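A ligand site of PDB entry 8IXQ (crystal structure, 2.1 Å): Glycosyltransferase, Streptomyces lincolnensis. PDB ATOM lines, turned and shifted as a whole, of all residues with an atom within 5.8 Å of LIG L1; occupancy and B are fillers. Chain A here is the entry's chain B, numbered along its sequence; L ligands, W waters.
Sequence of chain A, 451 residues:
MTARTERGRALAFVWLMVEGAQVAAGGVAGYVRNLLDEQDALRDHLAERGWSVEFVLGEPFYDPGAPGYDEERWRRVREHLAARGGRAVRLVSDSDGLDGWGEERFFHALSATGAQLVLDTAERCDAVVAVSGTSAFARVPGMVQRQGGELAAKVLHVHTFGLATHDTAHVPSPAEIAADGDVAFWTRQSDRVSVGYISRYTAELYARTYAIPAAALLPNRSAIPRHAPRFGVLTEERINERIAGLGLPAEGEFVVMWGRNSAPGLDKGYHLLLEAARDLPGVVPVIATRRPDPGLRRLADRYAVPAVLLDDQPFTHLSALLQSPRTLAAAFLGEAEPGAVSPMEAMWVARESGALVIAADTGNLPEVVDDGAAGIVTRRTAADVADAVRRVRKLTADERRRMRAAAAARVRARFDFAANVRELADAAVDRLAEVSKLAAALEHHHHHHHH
The side-chain carboxylate (OE2) of Glu 337 is in salt-bridge range of the side-chain amino group (NZ) of Lys 268 (2.6 Å). The backbone carbonyl oxygen (O) of Asp 311 sits at hydrogen-bond distance from the side-chain amide nitrogen (NE2) of Gln 313, 3.2 Å away. O of Gly 259 sits at hydrogen-bond distance from N of Arg 290 (3.0 Å). O of Ala 288 sits at hydrogen-bond distance from N of Gly 259 (3.0 Å). The guanidinium group of Arg 290 is in hydrogen-bond range of the backbone carbonyl oxygen of Ala 25 (2.9 Å). N of Asp 312 lies within hydrogen-bond range of O of Arg 290 (3.1 Å). N of Asp 312 lies within hydrogen-bond range of O of Thr 289 (3.1 Å).
Water W4 lies within hydrogen-bond range of O11 of LIG L1, O of Thr 289, N of Gln 313 and N of Asp 312. Water W7 bridges an oxygen (O6) of LIG L1 (2.8 Å) and the side-chain amino group of Lys 268 (3.0 Å). Water W5 lies within hydrogen-bond range of O1 of LIG L1 (2.8 Å) and N of Arg 260 (2.9 Å). Water W1 bridges the guanidinium group of Arg 33 (2.7 Å) and an oxygen (O9) of LIG L1 (3.0 Å). Water W11 lies within hydrogen-bond range of NH1 of Arg 290 (2.7 Å), OD1 of Asp 312 (2.8 Å), O of Gln 313 (3.0 Å) and N3 of LIG L1 (3.4 Å). Water W12 bridges S1 of LG2 L2 and O2 of LIG L1.
N of Ser 342 sits at hydrogen-bond distance from O6 of LIG L1, 3.1 Å away. An oxygen (O6) of LIG L1 lies within hydrogen-bond range of the side-chain hydroxyl of Ser 342 (2.5 Å). An oxygen (O10) of LIG L1 is in hydrogen-bond range of the side-chain carboxylate (OE1) of Glu 345, 2.6 Å away. O2 of LIG L1 is in salt-bridge range of NZ of Lys 268. The backbone carbonyl oxygen of Gln 313 is in hydrogen-bond range of a nitrogen (N3) of LIG L1, 2.8 Å away. An oxygen (O2) of LIG L1 lies within salt-bridge range of the guanidinium group (NH2) of Arg 260. O5 of LIG L1 sits at hydrogen-bond distance from N of Val 341. N of Gly 27 lies within hydrogen-bond range of O3 of LIG L1 (2.9 Å). The indole nitrogen (NE1) of Trp 258 is in hydrogen-bond range of an oxygen (O10) of LIG L1, 3.0 Å away. The guanidinium group of Arg 290 lies close to a nitrogen (N2) of LIG L1 (3.4 Å). The guanidinium group (NH1) of Arg 260 is in salt-bridge range of an oxygen (O2) of LG2 L2, 2.9 Å away.
N of Phe 315 lies close to N4 of LIG L1, 3.2 Å away. Residues that only touch LIG L1: Ala 25, Gly 26, Gly 259, Ala 288, Thr 289, Pro 314, Leu 318, Glu 337, Gly 339 and Ala 340. Of the 27 residues printed, 20 come within 4 Å of LIG L1.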
ATOM      1  N   ALA A  25      22.384  22.272 -12.037  1.00  0.00           N
ATOM      2  CA  ALA A  25      22.543  20.853 -11.742  1.00  0.00           C
ATOM      3  C   ALA A  25      21.227  20.093 -11.796  1.00  0.00           C
ATOM      4  O   ALA A  25      21.217  18.911 -12.134  1.00  0.00           O
ATOM      5  CB  ALA A  25      23.183  20.645 -10.362  1.00  0.00           C
ATOM      6  N   GLY A  26      20.116  20.732 -11.461  1.00  0.00           N
ATOM      7  CA  GLY A  26      18.892  19.979 -11.340  1.00  0.00           C
ATOM      8  C   GLY A  26      17.661  20.602 -11.952  1.00  0.00           C
ATOM      9  O   GLY A  26      17.756  21.395 -12.902  1.00  0.00           O
ATOM     10  N   GLY A  27      16.490  20.256 -11.390  1.00  0.00           N
ATOM     11  CA  GLY A  27      15.236  20.665 -12.005  1.00  0.00           C
ATOM     12  C   GLY A  27      14.977  22.158 -11.965  1.00  0.00           C
ATOM     13  O   GLY A  27      14.357  22.711 -12.870  1.00  0.00           O
ATOM     14  N   VAL A  28      15.441  22.837 -10.906  1.00  0.00           N
ATOM     15  CA  VAL A  28      15.270  24.289 -10.826  1.00  0.00           C
ATOM     16  C   VAL A  28      16.010  24.955 -11.977  1.00  0.00           C
ATOM     17  O   VAL A  28      15.457  25.816 -12.669  1.00  0.00           O
ATOM     18  CB  VAL A  28      15.751  24.823  -9.457  1.00  0.00           C
ATOM     19  CG1 VAL A  28      15.843  26.363  -9.467  1.00  0.00           C
ATOM     20  CG2 VAL A  28      14.813  24.370  -8.339  1.00  0.00           C
ATOM     21  N   GLY A  30      16.821  23.543 -14.821  1.00  0.00           N
ATOM     22  CA  GLY A  30      16.087  23.214 -16.035  1.00  0.00           C
ATOM     23  C   GLY A  30      14.863  24.094 -16.192  1.00  0.00           C
ATOM     24  O   GLY A  30      14.507  24.503 -17.297  1.00  0.00           O
ATOM     25  N   ARG A  33      15.940  27.454 -17.626  1.00  0.00           N
ATOM     26  CA  ARG A  33      16.204  27.316 -19.062  1.00  0.00           C
ATOM     27  C   ARG A  33      14.903  27.269 -19.841  1.00  0.00           C
ATOM     28  O   ARG A  33      14.742  27.959 -20.864  1.00  0.00           O
ATOM     29  CB  ARG A  33      17.033  26.071 -19.359  1.00  0.00           C
ATOM     30  CG  ARG A  33      17.366  25.921 -20.854  1.00  0.00           C
ATOM     31  CD  ARG A  33      18.244  24.706 -21.159  1.00  0.00           C
ATOM     32  NE  ARG A  33      17.643  23.487 -20.646  1.00  0.00           N
ATOM     33  CZ  ARG A  33      18.082  22.823 -19.575  1.00  0.00           C
ATOM     34  NH1 ARG A  33      19.179  23.194 -18.924  1.00  0.00           N
ATOM     35  NH2 ARG A  33      17.403  21.760 -19.149  1.00  0.00           N
ATOM     36  N   TRP A 258      19.454   8.521 -13.948  1.00  0.00           N
ATOM     37  CA  TRP A 258      20.362   9.660 -13.963  1.00  0.00           C
ATOM     38  C   TRP A 258      19.839  10.767 -13.062  1.00  0.00           C
ATOM     39  O   TRP A 258      18.648  10.812 -12.750  1.00  0.00           O
ATOM     40  CB  TRP A 258      20.590  10.193 -15.391  1.00  0.00           C
ATOM     41  CG  TRP A 258      19.484  11.049 -15.923  1.00  0.00           C
ATOM     42  CD1 TRP A 258      19.451  12.423 -15.959  1.00  0.00           C
ATOM     43  CD2 TRP A 258      18.257  10.603 -16.520  1.00  0.00           C
ATOM     44  NE1 TRP A 258      18.269  12.853 -16.530  1.00  0.00           N
ATOM     45  CE2 TRP A 258      17.520  11.755 -16.889  1.00  0.00           C
ATOM     46  CE3 TRP A 258      17.694   9.343 -16.767  1.00  0.00           C
ATOM     47  CZ2 TRP A 258      16.263  11.684 -17.485  1.00  0.00           C
ATOM     48  CZ3 TRP A 258      16.443   9.277 -17.384  1.00  0.00           C
ATOM     49  CH2 TRP A 258      15.742  10.442 -17.735  1.00  0.00           C
ATOM     50  N   GLY A 259      20.721  11.673 -12.665  1.00  0.00           N
ATOM     51  CA  GLY A 259      20.285  12.806 -11.871  1.00  0.00           C
ATOM     52  C   GLY A 259      21.390  13.324 -10.975  1.00  0.00           C
ATOM     53  O   GLY A 259      22.537  12.875 -11.028  1.00  0.00           O
ATOM     54  N   ARG A 260      21.028  14.314 -10.169  1.00  0.00           N
ATOM     55  CA  ARG A 260      21.901  14.789  -9.096  1.00  0.00           C
ATOM     56  C   ARG A 260      22.238  13.636  -8.161  1.00  0.00           C
ATOM     57  O   ARG A 260      21.406  12.768  -7.887  1.00  0.00           O
ATOM     58  CB  ARG A 260      21.224  15.910  -8.308  1.00  0.00           C
ATOM     59  CG  ARG A 260      21.045  17.190  -9.126  1.00  0.00           C
ATOM     60  CD  ARG A 260      20.541  18.330  -8.264  1.00  0.00           C
ATOM     61  NE  ARG A 260      19.172  18.078  -7.810  1.00  0.00           N
ATOM     62  CZ  ARG A 260      18.715  18.423  -6.610  1.00  0.00           C
ATOM     63  NH1 ARG A 260      19.491  19.058  -5.739  1.00  0.00           N
ATOM     64  NH2 ARG A 260      17.448  18.137  -6.277  1.00  0.00           N
ATOM     65  N   LEU A 266      18.016  14.193   0.092  1.00  0.00           N
ATOM     66  CA  LEU A 266      17.780  13.957  -1.329  1.00  0.00           C
ATOM     67  C   LEU A 266      18.217  12.517  -1.630  1.00  0.00           C
ATOM     68  O   LEU A 266      19.319  12.256  -2.130  1.00  0.00           O
ATOM     69  CB  LEU A 266      18.532  14.969  -2.193  1.00  0.00           C
ATOM     70  CG  LEU A 266      18.224  14.975  -3.695  1.00  0.00           C
ATOM     71  CD1 LEU A 266      16.833  15.521  -3.956  1.00  0.00           C
ATOM     72  CD2 LEU A 266      19.291  15.771  -4.442  1.00  0.00           C
ATOM     73  N   LYS A 268      17.877   9.799  -3.949  1.00  0.00           N
ATOM     74  CA  LYS A 268      17.392   9.515  -5.291  1.00  0.00           C
ATOM     75  C   LYS A 268      17.202   8.033  -5.534  1.00  0.00           C
ATOM     76  O   LYS A 268      16.730   7.654  -6.617  1.00  0.00           O
ATOM     77  CB  LYS A 268      18.351  10.106  -6.324  1.00  0.00           C
ATOM     78  CG  LYS A 268      18.263  11.625  -6.419  1.00  0.00           C
ATOM     79  CD  LYS A 268      17.168  12.052  -7.399  1.00  0.00           C
ATOM     80  CE  LYS A 268      17.079  13.582  -7.511  1.00  0.00           C
ATOM     81  NZ  LYS A 268      15.716  14.065  -7.978  1.00  0.00           N
ATOM     82  N   ALA A 288      23.888   7.458 -14.273  1.00  0.00           N
ATOM     83  CA  ALA A 288      24.630   8.653 -14.656  1.00  0.00           C
ATOM     84  C   ALA A 288      24.324   9.765 -13.659  1.00  0.00           C
ATOM     85  O   ALA A 288      23.240  10.349 -13.690  1.00  0.00           O
ATOM     86  CB  ALA A 288      24.259   9.079 -16.081  1.00  0.00           C
ATOM     87  N   THR A 289      25.255  10.070 -12.779  1.00  0.00           N
ATOM     88  CA  THR A 289      25.048  11.136 -11.816  1.00  0.00           C
ATOM     89  C   THR A 289      25.784  12.384 -12.284  1.00  0.00           C
ATOM     90  O   THR A 289      26.713  12.311 -13.081  1.00  0.00           O
ATOM     91  CB  THR A 289      25.524  10.718 -10.417  1.00  0.00           C
ATOM     92  OG1 THR A 289      26.787  10.060 -10.537  1.00  0.00           O
ATOM     93  CG2 THR A 289      24.541   9.745  -9.787  1.00  0.00           C
ATOM     94  N   ARG A 290      25.334  13.540 -11.794  1.00  0.00           N
ATOM     95  CA  ARG A 290      25.997  14.785 -12.164  1.00  0.00           C
ATOM     96  C   ARG A 290      27.493  14.714 -11.837  1.00  0.00           C
ATOM     97  O   ARG A 290      28.333  15.036 -12.665  1.00  0.00           O
ATOM     98  CB  ARG A 290      25.336  15.977 -11.450  1.00  0.00           C
ATOM     99  CG  ARG A 290      24.029  16.433 -12.103  1.00  0.00           C
ATOM    100  CD  ARG A 290      24.272  17.015 -13.501  1.00  0.00           C
ATOM    101  NE  ARG A 290      23.157  17.847 -13.942  1.00  0.00           N
ATOM    102  CZ  ARG A 290      23.034  18.372 -15.154  1.00  0.00           C
ATOM    103  NH1 ARG A 290      23.937  18.144 -16.117  1.00  0.00           N
ATOM    104  NH2 ARG A 290      21.999  19.158 -15.415  1.00  0.00           N
ATOM    105  N   ASP A 311      29.266   9.864 -15.165  1.00  0.00           N
ATOM    106  CA  ASP A 311      29.123  11.162 -14.546  1.00  0.00           C
ATOM    107  C   ASP A 311      29.213  12.250 -15.606  1.00  0.00           C
ATOM    108  O   ASP A 311      29.757  12.035 -16.694  1.00  0.00           O
ATOM    109  CB  ASP A 311      30.152  11.401 -13.429  1.00  0.00           C
ATOM    110  CG  ASP A 311      31.580  11.403 -13.938  1.00  0.00           C
ATOM    111  OD1 ASP A 311      32.059  12.459 -14.404  1.00  0.00           O
ATOM    112  OD2 ASP A 311      32.245  10.336 -13.865  1.00  0.00           O
ATOM    113  N   ASP A 312      28.650  13.406 -15.263  1.00  0.00           N
ATOM    114  CA  ASP A 312      28.642  14.602 -16.108  1.00  0.00           C
ATOM    115  C   ASP A 312      28.279  14.286 -17.560  1.00  0.00           C
ATOM    116  O   ASP A 312      28.920  14.741 -18.506  1.00  0.00           O
ATOM    117  CB  ASP A 312      29.988  15.329 -16.029  1.00  0.00           C
ATOM    118  CG  ASP A 312      29.909  16.742 -16.593  1.00  0.00           C
ATOM    119  OD1 ASP A 312      28.797  17.296 -16.629  1.00  0.00           O
ATOM    120  OD2 ASP A 312      30.946  17.270 -17.032  1.00  0.00           O
ATOM    121  N   GLN A 313      27.213  13.503 -17.739  1.00  0.00           N
ATOM    122  CA  GLN A 313      26.787  13.082 -19.076  1.00  0.00           C
ATOM    123  C   GLN A 313      25.926  14.158 -19.722  1.00  0.00           C
ATOM    124  O   GLN A 313      25.043  14.733 -19.073  1.00  0.00           O
ATOM    125  CB  GLN A 313      25.999  11.771 -18.999  1.00  0.00           C
ATOM    126  CG  GLN A 313      26.859  10.526 -18.778  1.00  0.00           C
ATOM    127  CD  GLN A 313      27.947  10.373 -19.848  1.00  0.00           C
ATOM    128  OE1 GLN A 313      27.656  10.259 -21.024  1.00  0.00           O
ATOM    129  NE2 GLN A 313      29.198  10.382 -19.420  1.00  0.00           N
ATOM    130  N   PRO A 314      26.145  14.450 -21.017  1.00  0.00           N
ATOM    131  CA  PRO A 314      25.242  15.353 -21.733  1.00  0.00           C
ATOM    132  C   PRO A 314      23.934  14.641 -22.065  1.00  0.00           C
ATOM    133  O   PRO A 314      23.873  13.414 -22.156  1.00  0.00           O
ATOM    134  CB  PRO A 314      26.027  15.695 -23.006  1.00  0.00           C
ATOM    135  CG  PRO A 314      26.837  14.434 -23.265  1.00  0.00           C
ATOM    136  CD  PRO A 314      27.229  13.937 -21.874  1.00  0.00           C
ATOM    137  N   PHE A 315      22.862  15.422 -22.210  1.00  0.00           N
ATOM    138  CA  PHE A 315      21.585  14.763 -22.440  1.00  0.00           C
ATOM    139  C   PHE A 315      21.542  14.011 -23.771  1.00  0.00           C
ATOM    140  O   PHE A 315      20.808  13.031 -23.904  1.00  0.00           O
ATOM    141  CB  PHE A 315      20.411  15.750 -22.367  1.00  0.00           C
ATOM    142  CG  PHE A 315      19.082  15.066 -22.209  1.00  0.00           C
ATOM    143  CD1 PHE A 315      18.608  14.714 -20.949  1.00  0.00           C
ATOM    144  CD2 PHE A 315      18.347  14.696 -23.318  1.00  0.00           C
ATOM    145  CE1 PHE A 315      17.413  14.039 -20.792  1.00  0.00           C
ATOM    146  CE2 PHE A 315      17.137  14.026 -23.170  1.00  0.00           C
ATOM    147  CZ  PHE A 315      16.677  13.691 -21.911  1.00  0.00           C
ATOM    148  N   LEU A 318      22.323  10.512 -22.664  1.00  0.00           N
ATOM    149  CA  LEU A 318      21.208   9.936 -21.919  1.00  0.00           C
ATOM    150  C   LEU A 318      20.055   9.606 -22.849  1.00  0.00           C
ATOM    151  O   LEU A 318      19.448   8.526 -22.744  1.00  0.00           O
ATOM    152  CB  LEU A 318      20.754  10.905 -20.825  1.00  0.00           C
ATOM    153  CG  LEU A 318      21.860  11.250 -19.825  1.00  0.00           C
ATOM    154  CD1 LEU A 318      21.370  12.310 -18.849  1.00  0.00           C
ATOM    155  CD2 LEU A 318      22.304   9.982 -19.108  1.00  0.00           C
ATOM    156  N   GLU A 337      10.065  12.911  -4.338  1.00  0.00           N
ATOM    157  CA  GLU A 337      10.201  13.987  -5.326  1.00  0.00           C
ATOM    158  C   GLU A 337       8.994  14.922  -5.237  1.00  0.00           C
ATOM    159  O   GLU A 337       7.859  14.452  -5.369  1.00  0.00           O
ATOM    160  CB  GLU A 337      10.299  13.413  -6.743  1.00  0.00           C
ATOM    161  CG  GLU A 337      11.439  12.431  -6.929  1.00  0.00           C
ATOM    162  CD  GLU A 337      12.783  13.146  -7.057  1.00  0.00           C
ATOM    163  OE1 GLU A 337      12.795  14.398  -7.113  1.00  0.00           O
ATOM    164  OE2 GLU A 337      13.809  12.451  -7.115  1.00  0.00           O
ATOM    165  N   GLY A 339       8.304  17.185  -7.489  1.00  0.00           N
ATOM    166  CA  GLY A 339       7.834  17.368  -8.858  1.00  0.00           C
ATOM    167  C   GLY A 339       8.906  17.083  -9.892  1.00  0.00           C
ATOM    168  O   GLY A 339       9.312  17.983 -10.628  1.00  0.00           O
ATOM    169  N   ALA A 340       9.378  15.836  -9.943  1.00  0.00           N
ATOM    170  CA  ALA A 340      10.494  15.499 -10.800  1.00  0.00           C
ATOM    171  C   ALA A 340      10.061  15.481 -12.261  1.00  0.00           C
ATOM    172  O   ALA A 340       9.010  14.915 -12.601  1.00  0.00           O
ATOM    173  CB  ALA A 340      11.073  14.135 -10.424  1.00  0.00           C
ATOM    174  N   VAL A 341      10.879  16.078 -13.129  1.00  0.00           N
ATOM    175  CA  VAL A 341      10.582  16.043 -14.551  1.00  0.00           C
ATOM    176  C   VAL A 341      11.380  14.974 -15.302  1.00  0.00           C
ATOM    177  O   VAL A 341      11.017  14.664 -16.444  1.00  0.00           O
ATOM    178  CB  VAL A 341      10.818  17.423 -15.213  1.00  0.00           C
ATOM    179  CG1 VAL A 341       9.990  18.489 -14.509  1.00  0.00           C
ATOM    180  CG2 VAL A 341      12.332  17.797 -15.223  1.00  0.00           C
ATOM    181  N   SER A 342      12.426  14.404 -14.693  1.00  0.00           N
ATOM    182  CA  SER A 342      13.196  13.372 -15.397  1.00  0.00           C
ATOM    183  C   SER A 342      12.360  12.186 -15.853  1.00  0.00           C
ATOM    184  O   SER A 342      12.567  11.722 -16.994  1.00  0.00           O
ATOM    185  CB  SER A 342      14.373  12.878 -14.523  1.00  0.00           C
ATOM    186  OG  SER A 342      15.282  13.924 -14.230  1.00  0.00           O
ATOM    187  N   PRO A 343      11.447  11.606 -15.052  1.00  0.00           N
ATOM    188  CA  PRO A 343      10.590  10.542 -15.596  1.00  0.00           C
ATOM    189  C   PRO A 343       9.789  11.010 -16.791  1.00  0.00           C
ATOM    190  O   PRO A 343       9.532  10.229 -17.714  1.00  0.00           O
ATOM    191  CB  PRO A 343       9.689  10.157 -14.413  1.00  0.00           C
ATOM    192  CG  PRO A 343       9.753  11.333 -13.481  1.00  0.00           C
ATOM    193  CD  PRO A 343      11.166  11.835 -13.628  1.00  0.00           C
ATOM    194  N   GLU A 345      10.871  13.245 -18.988  1.00  0.00           N
ATOM    195  CA  GLU A 345      11.828  13.213 -20.092  1.00  0.00           C
ATOM    196  C   GLU A 345      11.990  11.803 -20.665  1.00  0.00           C
ATOM    197  O   GLU A 345      12.046  11.621 -21.881  1.00  0.00           O
ATOM    198  CB  GLU A 345      13.181  13.765 -19.626  1.00  0.00           C
ATOM    199  CG  GLU A 345      13.137  15.262 -19.218  1.00  0.00           C
ATOM    200  CD  GLU A 345      14.391  15.739 -18.498  1.00  0.00           C
ATOM    201  OE1 GLU A 345      15.116  14.894 -17.900  1.00  0.00           O
ATOM    202  OE2 GLU A 345      14.645  16.958 -18.530  1.00  0.00           O
HETATM  203  P1  LIG L   1      15.692  17.490  -9.294  1.00  0.00           P
HETATM  204  O1  LIG L   1      17.103  17.618  -9.817  1.00  0.00           O
HETATM  205  O2  LIG L   1      15.627  16.759  -7.964  1.00  0.00           O
HETATM  206  O3  LIG L   1      14.935  18.796  -9.401  1.00  0.00           O
HETATM  207  O4  LIG L   1      14.950  16.427 -10.282  1.00  0.00           O
HETATM  208  P2  LIG L   1      14.201  16.647 -11.694  1.00  0.00           P
HETATM  209  O5  LIG L   1      12.902  17.422 -11.534  1.00  0.00           O
HETATM  210  O6  LIG L   1      14.208  15.302 -12.383  1.00  0.00           O
HETATM  211  O7  LIG L   1      15.182  17.573 -12.555  1.00  0.00           O
HETATM  212  C1  LIG L   1      16.449  17.095 -12.976  1.00  0.00           C
HETATM  213  C2  LIG L   1      16.792  17.865 -14.251  1.00  0.00           C
HETATM  214  O8  LIG L   1      18.208  17.906 -14.368  1.00  0.00           O
HETATM  215  C3  LIG L   1      16.268  17.063 -15.430  1.00  0.00           C
HETATM  216  O9  LIG L   1      16.078  17.969 -16.517  1.00  0.00           O
HETATM  217  C4  LIG L   1      17.444  16.168 -15.729  1.00  0.00           C
HETATM  218  O10 LIG L   1      17.408  15.693 -17.076  1.00  0.00           O
HETATM  219  C5  LIG L   1      18.608  17.108 -15.482  1.00  0.00           C
HETATM  220  N1  LIG L   1      19.804  16.301 -15.136  1.00  0.00           N
HETATM  221  C6  LIG L   1      20.033  15.768 -13.924  1.00  0.00           C
HETATM  222  N2  LIG L   1      21.197  15.069 -13.911  1.00  0.00           N
HETATM  223  C7  LIG L   1      21.719  15.169 -15.143  1.00  0.00           C
HETATM  224  C8  LIG L   1      22.940  14.678 -15.794  1.00  0.00           C
HETATM  225  O11 LIG L   1      23.764  13.977 -15.160  1.00  0.00           O
HETATM  226  N3  LIG L   1      23.123  15.009 -17.086  1.00  0.00           N
HETATM  227  C9  LIG L   1      22.238  15.769 -17.786  1.00  0.00           C
HETATM  228  N4  LIG L   1      22.492  16.068 -19.079  1.00  0.00           N
HETATM  229  N5  LIG L   1      21.090  16.268 -17.241  1.00  0.00           N
HETATM  230  C10 LIG L   1      20.794  15.998 -15.940  1.00  0.00           C
HETATM  231  O1  LG2 L   2      16.537  18.707  -3.433  1.00  0.00           O
HETATM  232  C1  LG2 L   2      17.319  19.473  -2.811  1.00  0.00           C
HETATM  233  O2  LG2 L   2      18.537  19.613  -3.044  1.00  0.00           O
HETATM  234  C2  LG2 L   2      16.690  20.358  -1.700  1.00  0.00           C
HETATM  235  N1  LG2 L   2      17.246  20.055  -0.352  1.00  0.00           N
HETATM  236  C3  LG2 L   2      16.274  20.548   0.628  1.00  0.00           C
HETATM  237  C4  LG2 L   2      17.379  18.599  -0.173  1.00  0.00           C
HETATM  238  C5  LG2 L   2      18.567  20.681  -0.098  1.00  0.00           C
HETATM  239  C6  LG2 L   2      16.791  21.838  -2.174  1.00  0.00           C
HETATM  240  C7  LG2 L   2      16.058  21.843  -3.521  1.00  0.00           C
HETATM  241  N2  LG2 L   2      14.738  21.722  -3.637  1.00  0.00           N
HETATM  242  C8  LG2 L   2      14.481  21.735  -4.936  1.00  0.00           C
HETATM  243  S1  LG2 L   2      12.818  21.585  -5.629  1.00  0.00           S
HETATM  244  N3  LG2 L   2      15.608  21.852  -5.639  1.00  0.00           N
HETATM  245  C9  LG2 L   2      16.617  21.910  -4.741  1.00  0.00           C
HETATM  246  O   HOH W   1      18.155  19.918 -17.370  1.00  0.00           O
HETATM  247  O   HOH W   2      19.422  20.911 -14.981  1.00  0.00           O
HETATM  248  O   HOH W   3      11.836  20.428 -11.692  1.00  0.00           O
HETATM  249  O   HOH W   4      25.770  12.181 -15.706  1.00  0.00           O
HETATM  250  O   HOH W   5      18.224  15.092 -10.402  1.00  0.00           O
HETATM  251  O   HOH W   6      15.940  21.163  -8.381  1.00  0.00           O
HETATM  252  O   HOH W   7      15.037  13.157 -10.774  1.00  0.00           O
HETATM  253  O   HOH W   8      12.323  18.859  -9.360  1.00  0.00           O
HETATM  254  O   HOH W   9      19.016  17.929 -19.079  1.00  0.00           O
HETATM  255  O   HOH W  10      14.561  20.441 -16.416  1.00  0.00           O
HETATM  256  O   HOH W  11      26.061  16.684 -17.015  1.00  0.00           O
HETATM  257  O   HOH W  12      13.046  18.485  -6.542  1.00  0.00           O
